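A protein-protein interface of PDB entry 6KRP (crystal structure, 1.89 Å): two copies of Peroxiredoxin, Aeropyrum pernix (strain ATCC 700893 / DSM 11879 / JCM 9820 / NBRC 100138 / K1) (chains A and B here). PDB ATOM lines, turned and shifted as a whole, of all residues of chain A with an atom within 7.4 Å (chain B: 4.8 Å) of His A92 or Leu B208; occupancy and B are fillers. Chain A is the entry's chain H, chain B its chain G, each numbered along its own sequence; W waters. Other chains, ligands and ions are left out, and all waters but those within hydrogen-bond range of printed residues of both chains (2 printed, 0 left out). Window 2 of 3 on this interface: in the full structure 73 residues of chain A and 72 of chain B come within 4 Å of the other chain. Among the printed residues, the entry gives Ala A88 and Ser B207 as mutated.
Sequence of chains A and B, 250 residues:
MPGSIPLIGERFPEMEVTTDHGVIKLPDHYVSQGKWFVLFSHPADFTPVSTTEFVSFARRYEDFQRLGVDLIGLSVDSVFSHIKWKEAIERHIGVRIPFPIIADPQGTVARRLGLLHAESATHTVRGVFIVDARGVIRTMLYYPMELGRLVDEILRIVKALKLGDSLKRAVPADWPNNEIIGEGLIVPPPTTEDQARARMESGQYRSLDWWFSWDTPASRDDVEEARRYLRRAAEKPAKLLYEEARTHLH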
ATOM      1  N   THR A  51     -26.400 -18.554 -27.303  1.00  0.00           N
ATOM      2  CA  THR A  51     -26.085 -20.005 -27.373  1.00  0.00           C
ATOM      3  C   THR A  51     -27.070 -20.813 -26.497  1.00  0.00           C
ATOM      4  O   THR A  51     -27.631 -21.804 -26.992  1.00  0.00           O
ATOM      5  CB  THR A  51     -24.608 -20.276 -27.031  1.00  0.00           C
ATOM      6  OG1 THR A  51     -23.770 -19.567 -27.963  1.00  0.00           O
ATOM      7  CG2 THR A  51     -24.269 -21.739 -27.145  1.00  0.00           C
ATOM      8  N   LYS A  86     -22.653 -22.806 -35.315  1.00  0.00           N
ATOM      9  CA  LYS A  86     -23.383 -24.089 -35.109  1.00  0.00           C
ATOM     10  C   LYS A  86     -22.377 -25.239 -34.928  1.00  0.00           C
ATOM     11  O   LYS A  86     -22.639 -26.158 -34.109  1.00  0.00           O
ATOM     12  CB  LYS A  86     -24.418 -24.224 -36.227  1.00  0.00           C
ATOM     13  CG  LYS A  86     -25.642 -23.363 -35.959  1.00  0.00           C
ATOM     14  CD  LYS A  86     -26.667 -23.147 -37.081  1.00  0.00           C
ATOM     15  CE  LYS A  86     -27.105 -24.400 -37.781  1.00  0.00           C
ATOM     16  NZ  LYS A  86     -28.284 -24.124 -38.649  1.00  0.00           N
ATOM     17  N   GLU A  87     -21.262 -25.219 -35.661  1.00  0.00           N
ATOM     18  CA  GLU A  87     -20.178 -26.221 -35.507  1.00  0.00           C
ATOM     19  C   GLU A  87     -19.639 -26.156 -34.066  1.00  0.00           C
ATOM     20  O   GLU A  87     -19.517 -27.218 -33.441  1.00  0.00           O
ATOM     21  CB  GLU A  87     -19.157 -25.977 -36.607  1.00  0.00           C
ATOM     22  CG  GLU A  87     -17.836 -26.676 -36.457  1.00  0.00           C
ATOM     23  CD  GLU A  87     -16.904 -26.257 -37.593  1.00  0.00           C
ATOM     24  OE1 GLU A  87     -15.694 -26.347 -37.402  1.00  0.00           O
ATOM     25  OE2 GLU A  87     -17.418 -25.812 -38.670  1.00  0.00           O
ATOM     26  N   ALA A  88     -19.338 -24.969 -33.548  1.00  0.00           N
ATOM     27  CA  ALA A  88     -18.795 -24.762 -32.194  1.00  0.00           C
ATOM     28  C   ALA A  88     -19.783 -25.264 -31.123  1.00  0.00           C
ATOM     29  O   ALA A  88     -19.338 -25.875 -30.107  1.00  0.00           O
ATOM     30  CB  ALA A  88     -18.435 -23.316 -31.998  1.00  0.00           C
ATOM     31  N   ILE A  89     -21.074 -25.041 -31.326  1.00  0.00           N
ATOM     32  CA  ILE A  89     -22.102 -25.504 -30.358  1.00  0.00           C
ATOM     33  C   ILE A  89     -22.107 -27.041 -30.380  1.00  0.00           C
ATOM     34  O   ILE A  89     -22.126 -27.665 -29.290  1.00  0.00           O
ATOM     35  CB  ILE A  89     -23.466 -24.890 -30.695  1.00  0.00           C
ATOM     36  CG1 ILE A  89     -23.529 -23.388 -30.390  1.00  0.00           C
ATOM     37  CG2 ILE A  89     -24.564 -25.658 -29.986  1.00  0.00           C
ATOM     38  CD1 ILE A  89     -24.809 -22.735 -30.938  1.00  0.00           C
ATOM     39  N   GLU A  90     -22.007 -27.652 -31.557  1.00  0.00           N
ATOM     40  CA  GLU A  90     -21.972 -29.133 -31.672  1.00  0.00           C
ATOM     41  C   GLU A  90     -20.703 -29.674 -31.018  1.00  0.00           C
ATOM     42  O   GLU A  90     -20.831 -30.638 -30.209  1.00  0.00           O
ATOM     43  CB  GLU A  90     -22.059 -29.667 -33.101  1.00  0.00           C
ATOM     44  CG  GLU A  90     -22.518 -31.117 -33.130  1.00  0.00           C
ATOM     45  CD  GLU A  90     -22.985 -31.660 -34.468  1.00  0.00           C
ATOM     46  OE1 GLU A  90     -23.892 -32.522 -34.463  1.00  0.00           O
ATOM     47  OE2 GLU A  90     -22.424 -31.256 -35.509  1.00  0.00           O
ATOM     48  N   ARG A  91     -19.544 -29.074 -31.305  1.00  0.00           N
ATOM     49  CA  ARG A  91     -18.242 -29.525 -30.746  1.00  0.00           C
ATOM     50  C   ARG A  91     -18.222 -29.377 -29.213  1.00  0.00           C
ATOM     51  O   ARG A  91     -17.821 -30.344 -28.558  1.00  0.00           O
ATOM     52  CB  ARG A  91     -17.065 -28.782 -31.387  1.00  0.00           C
ATOM     53  CG  ARG A  91     -15.711 -29.443 -31.147  1.00  0.00           C
ATOM     54  CD  ARG A  91     -15.086 -30.051 -32.412  1.00  0.00           C
ATOM     55  NE  ARG A  91     -14.304 -29.075 -33.190  1.00  0.00           N
ATOM     56  CZ  ARG A  91     -14.670 -28.487 -34.344  1.00  0.00           C
ATOM     57  NH1 ARG A  91     -15.819 -28.774 -34.935  1.00  0.00           N
ATOM     58  NH2 ARG A  91     -13.864 -27.612 -34.921  1.00  0.00           N
ATOM     59  N   HIS A  92     -18.626 -28.240 -28.646  1.00  0.00           N
ATOM     60  CA  HIS A  92     -18.416 -27.907 -27.211  1.00  0.00           C
ATOM     61  C   HIS A  92     -19.603 -28.306 -26.317  1.00  0.00           C
ATOM     62  O   HIS A  92     -19.395 -28.397 -25.115  1.00  0.00           O
ATOM     63  CB  HIS A  92     -18.086 -26.428 -27.041  1.00  0.00           C
ATOM     64  CG  HIS A  92     -16.745 -26.089 -27.599  1.00  0.00           C
ATOM     65  ND1 HIS A  92     -15.576 -26.356 -26.911  1.00  0.00           N
ATOM     66  CD2 HIS A  92     -16.374 -25.592 -28.804  1.00  0.00           C
ATOM     67  CE1 HIS A  92     -14.546 -26.011 -27.660  1.00  0.00           C
ATOM     68  NE2 HIS A  92     -15.005 -25.525 -28.820  1.00  0.00           N
ATOM     69  N   ILE A  93     -20.812 -28.466 -26.850  1.00  0.00           N
ATOM     70  CA  ILE A  93     -22.031 -28.717 -26.027  1.00  0.00           C
ATOM     71  C   ILE A  93     -22.656 -30.052 -26.418  1.00  0.00           C
ATOM     72  O   ILE A  93     -23.470 -30.535 -25.629  1.00  0.00           O
ATOM     73  CB  ILE A  93     -23.014 -27.534 -26.175  1.00  0.00           C
ATOM     74  CG1 ILE A  93     -22.315 -26.227 -25.818  1.00  0.00           C
ATOM     75  CG2 ILE A  93     -24.268 -27.729 -25.350  1.00  0.00           C
ATOM     76  CD1 ILE A  93     -23.182 -25.008 -25.924  1.00  0.00           C
ATOM     77  N   GLY A  94     -22.348 -30.587 -27.604  1.00  0.00           N
ATOM     78  CA  GLY A  94     -22.894 -31.867 -28.099  1.00  0.00           C
ATOM     79  C   GLY A  94     -24.310 -31.724 -28.606  1.00  0.00           C
ATOM     80  O   GLY A  94     -25.018 -32.735 -28.687  1.00  0.00           O
ATOM     81  N   VAL A  95     -24.730 -30.515 -28.983  1.00  0.00           N
ATOM     82  CA  VAL A  95     -26.114 -30.278 -29.495  1.00  0.00           C
ATOM     83  C   VAL A  95     -26.047 -29.727 -30.910  1.00  0.00           C
ATOM     84  O   VAL A  95     -25.378 -28.707 -31.097  1.00  0.00           O
ATOM     85  CB  VAL A  95     -26.889 -29.330 -28.566  1.00  0.00           C
ATOM     86  CG1 VAL A  95     -28.285 -29.043 -29.108  1.00  0.00           C
ATOM     87  CG2 VAL A  95     -27.003 -29.930 -27.176  1.00  0.00           C
ATOM     88  N   LEU A 241     -25.755 -30.095 -19.363  1.00  0.00           N
ATOM     89  CA  LEU A 241     -25.005 -30.390 -20.617  1.00  0.00           C
ATOM     90  C   LEU A 241     -23.519 -29.997 -20.464  1.00  0.00           C
ATOM     91  O   LEU A 241     -22.686 -30.638 -21.134  1.00  0.00           O
ATOM     92  CB  LEU A 241     -25.662 -29.692 -21.817  1.00  0.00           C
ATOM     93  CG  LEU A 241     -26.972 -30.329 -22.285  1.00  0.00           C
ATOM     94  CD1 LEU A 241     -27.787 -29.384 -23.139  1.00  0.00           C
ATOM     95  CD2 LEU A 241     -26.702 -31.598 -23.058  1.00  0.00           C
ATOM     96  N   TYR A 242     -23.163 -29.008 -19.642  1.00  0.00           N
ATOM     97  CA  TYR A 242     -21.737 -28.610 -19.480  1.00  0.00           C
ATOM     98  C   TYR A 242     -20.954 -29.769 -18.843  1.00  0.00           C
ATOM     99  O   TYR A 242     -19.838 -30.000 -19.324  1.00  0.00           O
ATOM    100  CB  TYR A 242     -21.563 -27.299 -18.717  1.00  0.00           C
ATOM    101  CG  TYR A 242     -21.249 -27.405 -17.251  1.00  0.00           C
ATOM    102  CD1 TYR A 242     -19.943 -27.489 -16.793  1.00  0.00           C
ATOM    103  CD2 TYR A 242     -22.269 -27.344 -16.311  1.00  0.00           C
ATOM    104  CE1 TYR A 242     -19.666 -27.540 -15.431  1.00  0.00           C
ATOM    105  CE2 TYR A 242     -22.008 -27.391 -14.950  1.00  0.00           C
ATOM    106  CZ  TYR A 242     -20.703 -27.493 -14.504  1.00  0.00           C
ATOM    107  OH  TYR A 242     -20.507 -27.536 -13.153  1.00  0.00           O
ATOM    108  N   GLU A 243     -21.515 -30.479 -17.849  1.00  0.00           N
ATOM    109  CA  GLU A 243     -20.885 -31.690 -17.235  1.00  0.00           C
ATOM    110  C   GLU A 243     -20.768 -32.839 -18.259  1.00  0.00           C
ATOM    111  O   GLU A 243     -19.768 -33.554 -18.201  1.00  0.00           O
ATOM    112  CB  GLU A 243     -21.663 -32.180 -16.011  1.00  0.00           C
ATOM    113  CG  GLU A 243     -20.837 -32.211 -14.735  1.00  0.00           C
ATOM    114  CD  GLU A 243     -20.950 -30.976 -13.857  1.00  0.00           C
ATOM    115  OE1 GLU A 243     -22.087 -30.546 -13.581  1.00  0.00           O
ATOM    116  OE2 GLU A 243     -19.901 -30.466 -13.432  1.00  0.00           O
ATOM    117  N   GLU A 244     -21.762 -33.033 -19.133  1.00  0.00           N
ATOM    118  CA  GLU A 244     -21.811 -34.130 -20.150  1.00  0.00           C
ATOM    119  C   GLU A 244     -20.774 -33.897 -21.260  1.00  0.00           C
ATOM    120  O   GLU A 244     -20.409 -34.891 -21.923  1.00  0.00           O
ATOM    121  CB  GLU A 244     -23.212 -34.245 -20.759  1.00  0.00           C
ATOM    122  CG  GLU A 244     -24.270 -34.671 -19.755  1.00  0.00           C
ATOM    123  CD  GLU A 244     -25.662 -34.884 -20.332  1.00  0.00           C
ATOM    124  OE1 GLU A 244     -25.962 -34.310 -21.401  1.00  0.00           O
ATOM    125  OE2 GLU A 244     -26.444 -35.629 -19.716  1.00  0.00           O
ATOM    126  N   ALA A 245     -20.357 -32.639 -21.468  1.00  0.00           N
ATOM    127  CA  ALA A 245     -19.244 -32.217 -22.353  1.00  0.00           C
ATOM    128  C   ALA A 245     -17.965 -32.070 -21.519  1.00  0.00           C
ATOM    129  O   ALA A 245     -16.966 -32.746 -21.756  1.00  0.00           O
ATOM    130  CB  ALA A 245     -19.597 -30.923 -23.051  1.00  0.00           C
ATOM    131  N   ILE B 180     -27.896 -26.158 -19.855  1.00  0.00           N
ATOM    132  CA  ILE B 180     -26.404 -26.213 -19.969  1.00  0.00           C
ATOM    133  C   ILE B 180     -25.799 -25.912 -18.601  1.00  0.00           C
ATOM    134  O   ILE B 180     -24.879 -26.639 -18.206  1.00  0.00           O
ATOM    135  CB  ILE B 180     -25.834 -25.241 -21.018  1.00  0.00           C
ATOM    136  CG1 ILE B 180     -26.477 -25.442 -22.389  1.00  0.00           C
ATOM    137  CG2 ILE B 180     -24.312 -25.408 -21.082  1.00  0.00           C
ATOM    138  CD1 ILE B 180     -26.137 -24.335 -23.379  1.00  0.00           C
ATOM    139  N   ARG B 206     -15.852 -21.041 -14.747  1.00  0.00           N
ATOM    140  CA  ARG B 206     -16.169 -22.188 -15.615  1.00  0.00           C
ATOM    141  C   ARG B 206     -16.460 -21.632 -17.022  1.00  0.00           C
ATOM    142  O   ARG B 206     -17.085 -20.569 -17.121  1.00  0.00           O
ATOM    143  CB  ARG B 206     -17.313 -22.981 -14.986  1.00  0.00           C
ATOM    144  CG  ARG B 206     -16.835 -24.018 -13.977  1.00  0.00           C
ATOM    145  CD  ARG B 206     -17.966 -24.769 -13.316  1.00  0.00           C
ATOM    146  NE  ARG B 206     -18.861 -23.856 -12.622  1.00  0.00           N
ATOM    147  CZ  ARG B 206     -18.825 -23.577 -11.319  1.00  0.00           C
ATOM    148  NH1 ARG B 206     -17.916 -24.139 -10.541  1.00  0.00           N
ATOM    149  NH2 ARG B 206     -19.702 -22.733 -10.795  1.00  0.00           N
ATOM    150  N   SER B 207     -15.937 -22.264 -18.056  1.00  0.00           N
ATOM    151  CA  SER B 207     -15.941 -21.758 -19.461  1.00  0.00           C
ATOM    152  C   SER B 207     -16.149 -22.944 -20.393  1.00  0.00           C
ATOM    153  O   SER B 207     -15.596 -23.978 -20.079  1.00  0.00           O
ATOM    154  CB  SER B 207     -14.652 -21.061 -19.817  1.00  0.00           C
ATOM    155  OG  SER B 207     -14.592 -19.768 -19.210  1.00  0.00           O
ATOM    156  N   LEU B 208     -16.871 -22.783 -21.500  1.00  0.00           N
ATOM    157  CA  LEU B 208     -16.875 -23.770 -22.605  1.00  0.00           C
ATOM    158  C   LEU B 208     -15.847 -23.305 -23.645  1.00  0.00           C
ATOM    159  O   LEU B 208     -15.277 -24.143 -24.320  1.00  0.00           O
ATOM    160  CB  LEU B 208     -18.289 -23.861 -23.181  1.00  0.00           C
ATOM    161  CG  LEU B 208     -19.186 -24.963 -22.619  1.00  0.00           C
ATOM    162  CD1 LEU B 208     -18.821 -25.337 -21.203  1.00  0.00           C
ATOM    163  CD2 LEU B 208     -20.643 -24.542 -22.709  1.00  0.00           C
ATOM    164  N   ASP B 209     -15.632 -21.995 -23.737  1.00  0.00           N
ATOM    165  CA  ASP B 209     -14.597 -21.350 -24.591  1.00  0.00           C
ATOM    166  C   ASP B 209     -14.559 -19.893 -24.148  1.00  0.00           C
ATOM    167  O   ASP B 209     -15.280 -19.532 -23.166  1.00  0.00           O
ATOM    168  CB  ASP B 209     -14.914 -21.566 -26.079  1.00  0.00           C
ATOM    169  CG  ASP B 209     -13.751 -21.398 -27.065  1.00  0.00           C
ATOM    170  OD1 ASP B 209     -12.637 -21.023 -26.645  1.00  0.00           O
ATOM    171  OD2 ASP B 209     -13.983 -21.612 -28.247  1.00  0.00           O
ATOM    172  N   PHE B 212     -17.888 -17.983 -23.623  1.00  0.00           N
ATOM    173  CA  PHE B 212     -18.981 -18.616 -22.801  1.00  0.00           C
ATOM    174  C   PHE B 212     -18.428 -18.969 -21.422  1.00  0.00           C
ATOM    175  O   PHE B 212     -17.836 -20.068 -21.286  1.00  0.00           O
ATOM    176  CB  PHE B 212     -19.513 -19.888 -23.488  1.00  0.00           C
ATOM    177  CG  PHE B 212     -20.857 -20.386 -22.968  1.00  0.00           C
ATOM    178  CD1 PHE B 212     -21.075 -20.617 -21.621  1.00  0.00           C
ATOM    179  CD2 PHE B 212     -21.898 -20.693 -23.832  1.00  0.00           C
ATOM    180  CE1 PHE B 212     -22.305 -21.077 -21.154  1.00  0.00           C
ATOM    181  CE2 PHE B 212     -23.128 -21.134 -23.363  1.00  0.00           C
ATOM    182  CZ  PHE B 212     -23.328 -21.332 -22.021  1.00  0.00           C
ATOM    183  N   TRP B 214     -19.395 -18.671 -17.007  1.00  0.00           N
ATOM    184  CA  TRP B 214     -20.468 -18.448 -16.002  1.00  0.00           C
ATOM    185  C   TRP B 214     -19.960 -18.838 -14.604  1.00  0.00           C
ATOM    186  O   TRP B 214     -18.896 -19.504 -14.502  1.00  0.00           O
ATOM    187  CB  TRP B 214     -21.717 -19.254 -16.394  1.00  0.00           C
ATOM    188  CG  TRP B 214     -21.590 -20.685 -16.000  1.00  0.00           C
ATOM    189  CD1 TRP B 214     -22.071 -21.273 -14.858  1.00  0.00           C
ATOM    190  CD2 TRP B 214     -20.929 -21.713 -16.731  1.00  0.00           C
ATOM    191  NE1 TRP B 214     -21.710 -22.580 -14.824  1.00  0.00           N
ATOM    192  CE2 TRP B 214     -21.025 -22.879 -15.959  1.00  0.00           C
ATOM    193  CE3 TRP B 214     -20.251 -21.748 -17.940  1.00  0.00           C
ATOM    194  CZ2 TRP B 214     -20.467 -24.078 -16.368  1.00  0.00           C
ATOM    195  CZ3 TRP B 214     -19.691 -22.930 -18.346  1.00  0.00           C
ATOM    196  CH2 TRP B 214     -19.790 -24.077 -17.562  1.00  0.00           C
HETATM  197  O   HOH W   1     -15.831 -22.344 -29.852  1.00  0.00           O
HETATM  198  O   HOH W   2     -12.526 -23.681 -29.130  1.00  0.00           O
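O of Leu B208 lies within hydrogen-bond range of ND1 of His A92.
The backbone NH (N) of Tyr A242 is in hydrogen-bond range of the backbone carbonyl oxygen (O) of Ile B180 (3.3 Å).
Phe B212 touches Thr A51.
CD1 of Ile B180 touches CD1 of Ile A93, at 3.96 Å.
CG1 of Ile A93 touches CD2 of Leu B208 (3.9 Å).
Leu A241 touches Ile B180.
OH of Tyr A242 touches CD of Arg B206, at 3.8 Å.
Trp B214 touches Tyr A242.
No position is printed for both chains.
Water W1 bridges the side-chain carboxylate (OD2) of Asp B209 and a ring nitrogen (NE2) of His A92.
Water W2 bridges the side-chain carboxylate of Asp B209 (2.7 Å) and a ring nitrogen (NE2) of His A92 (3.1 Å).
N of Trp B214 is in hydrogen-bond range of O of Arg B206 (3.0 Å).
OH of Tyr A242 sits at hydrogen-bond distance from OE2 of Glu A243 (3.0 Å).
Hydrophobic or aromatic side chains of chain A within 4 Å of the printed part of chain B: His A92, Ile A93 and Tyr A242.
Of the 7 printed residues of chain B, 5 touch a printed residue of chain A.
Among the printed residues, no Asp or Glu carboxylate lies within 4 Å of a Lys or Arg side-chain nitrogen of the other chain.
Of chain B, only Leu B208 comes within 4 Å of His A92.
Leu B208 touches just these residues of chain A: His A92 and Ile A93.
Of the printed residues of chain B, Tyr A242 touches Ile B180, Arg B206 and Trp B214.
Printed residues of chain B within 4 Å of Ile A93: Ile B180 and Leu B208.
Glu A244 touches none of the printed residues of chain B.
Asp B209 touches none of the printed residues of chain A.
The nearest printed residue of chain B that does not touch Ile A93 is Phe B212 (4.6 Å).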
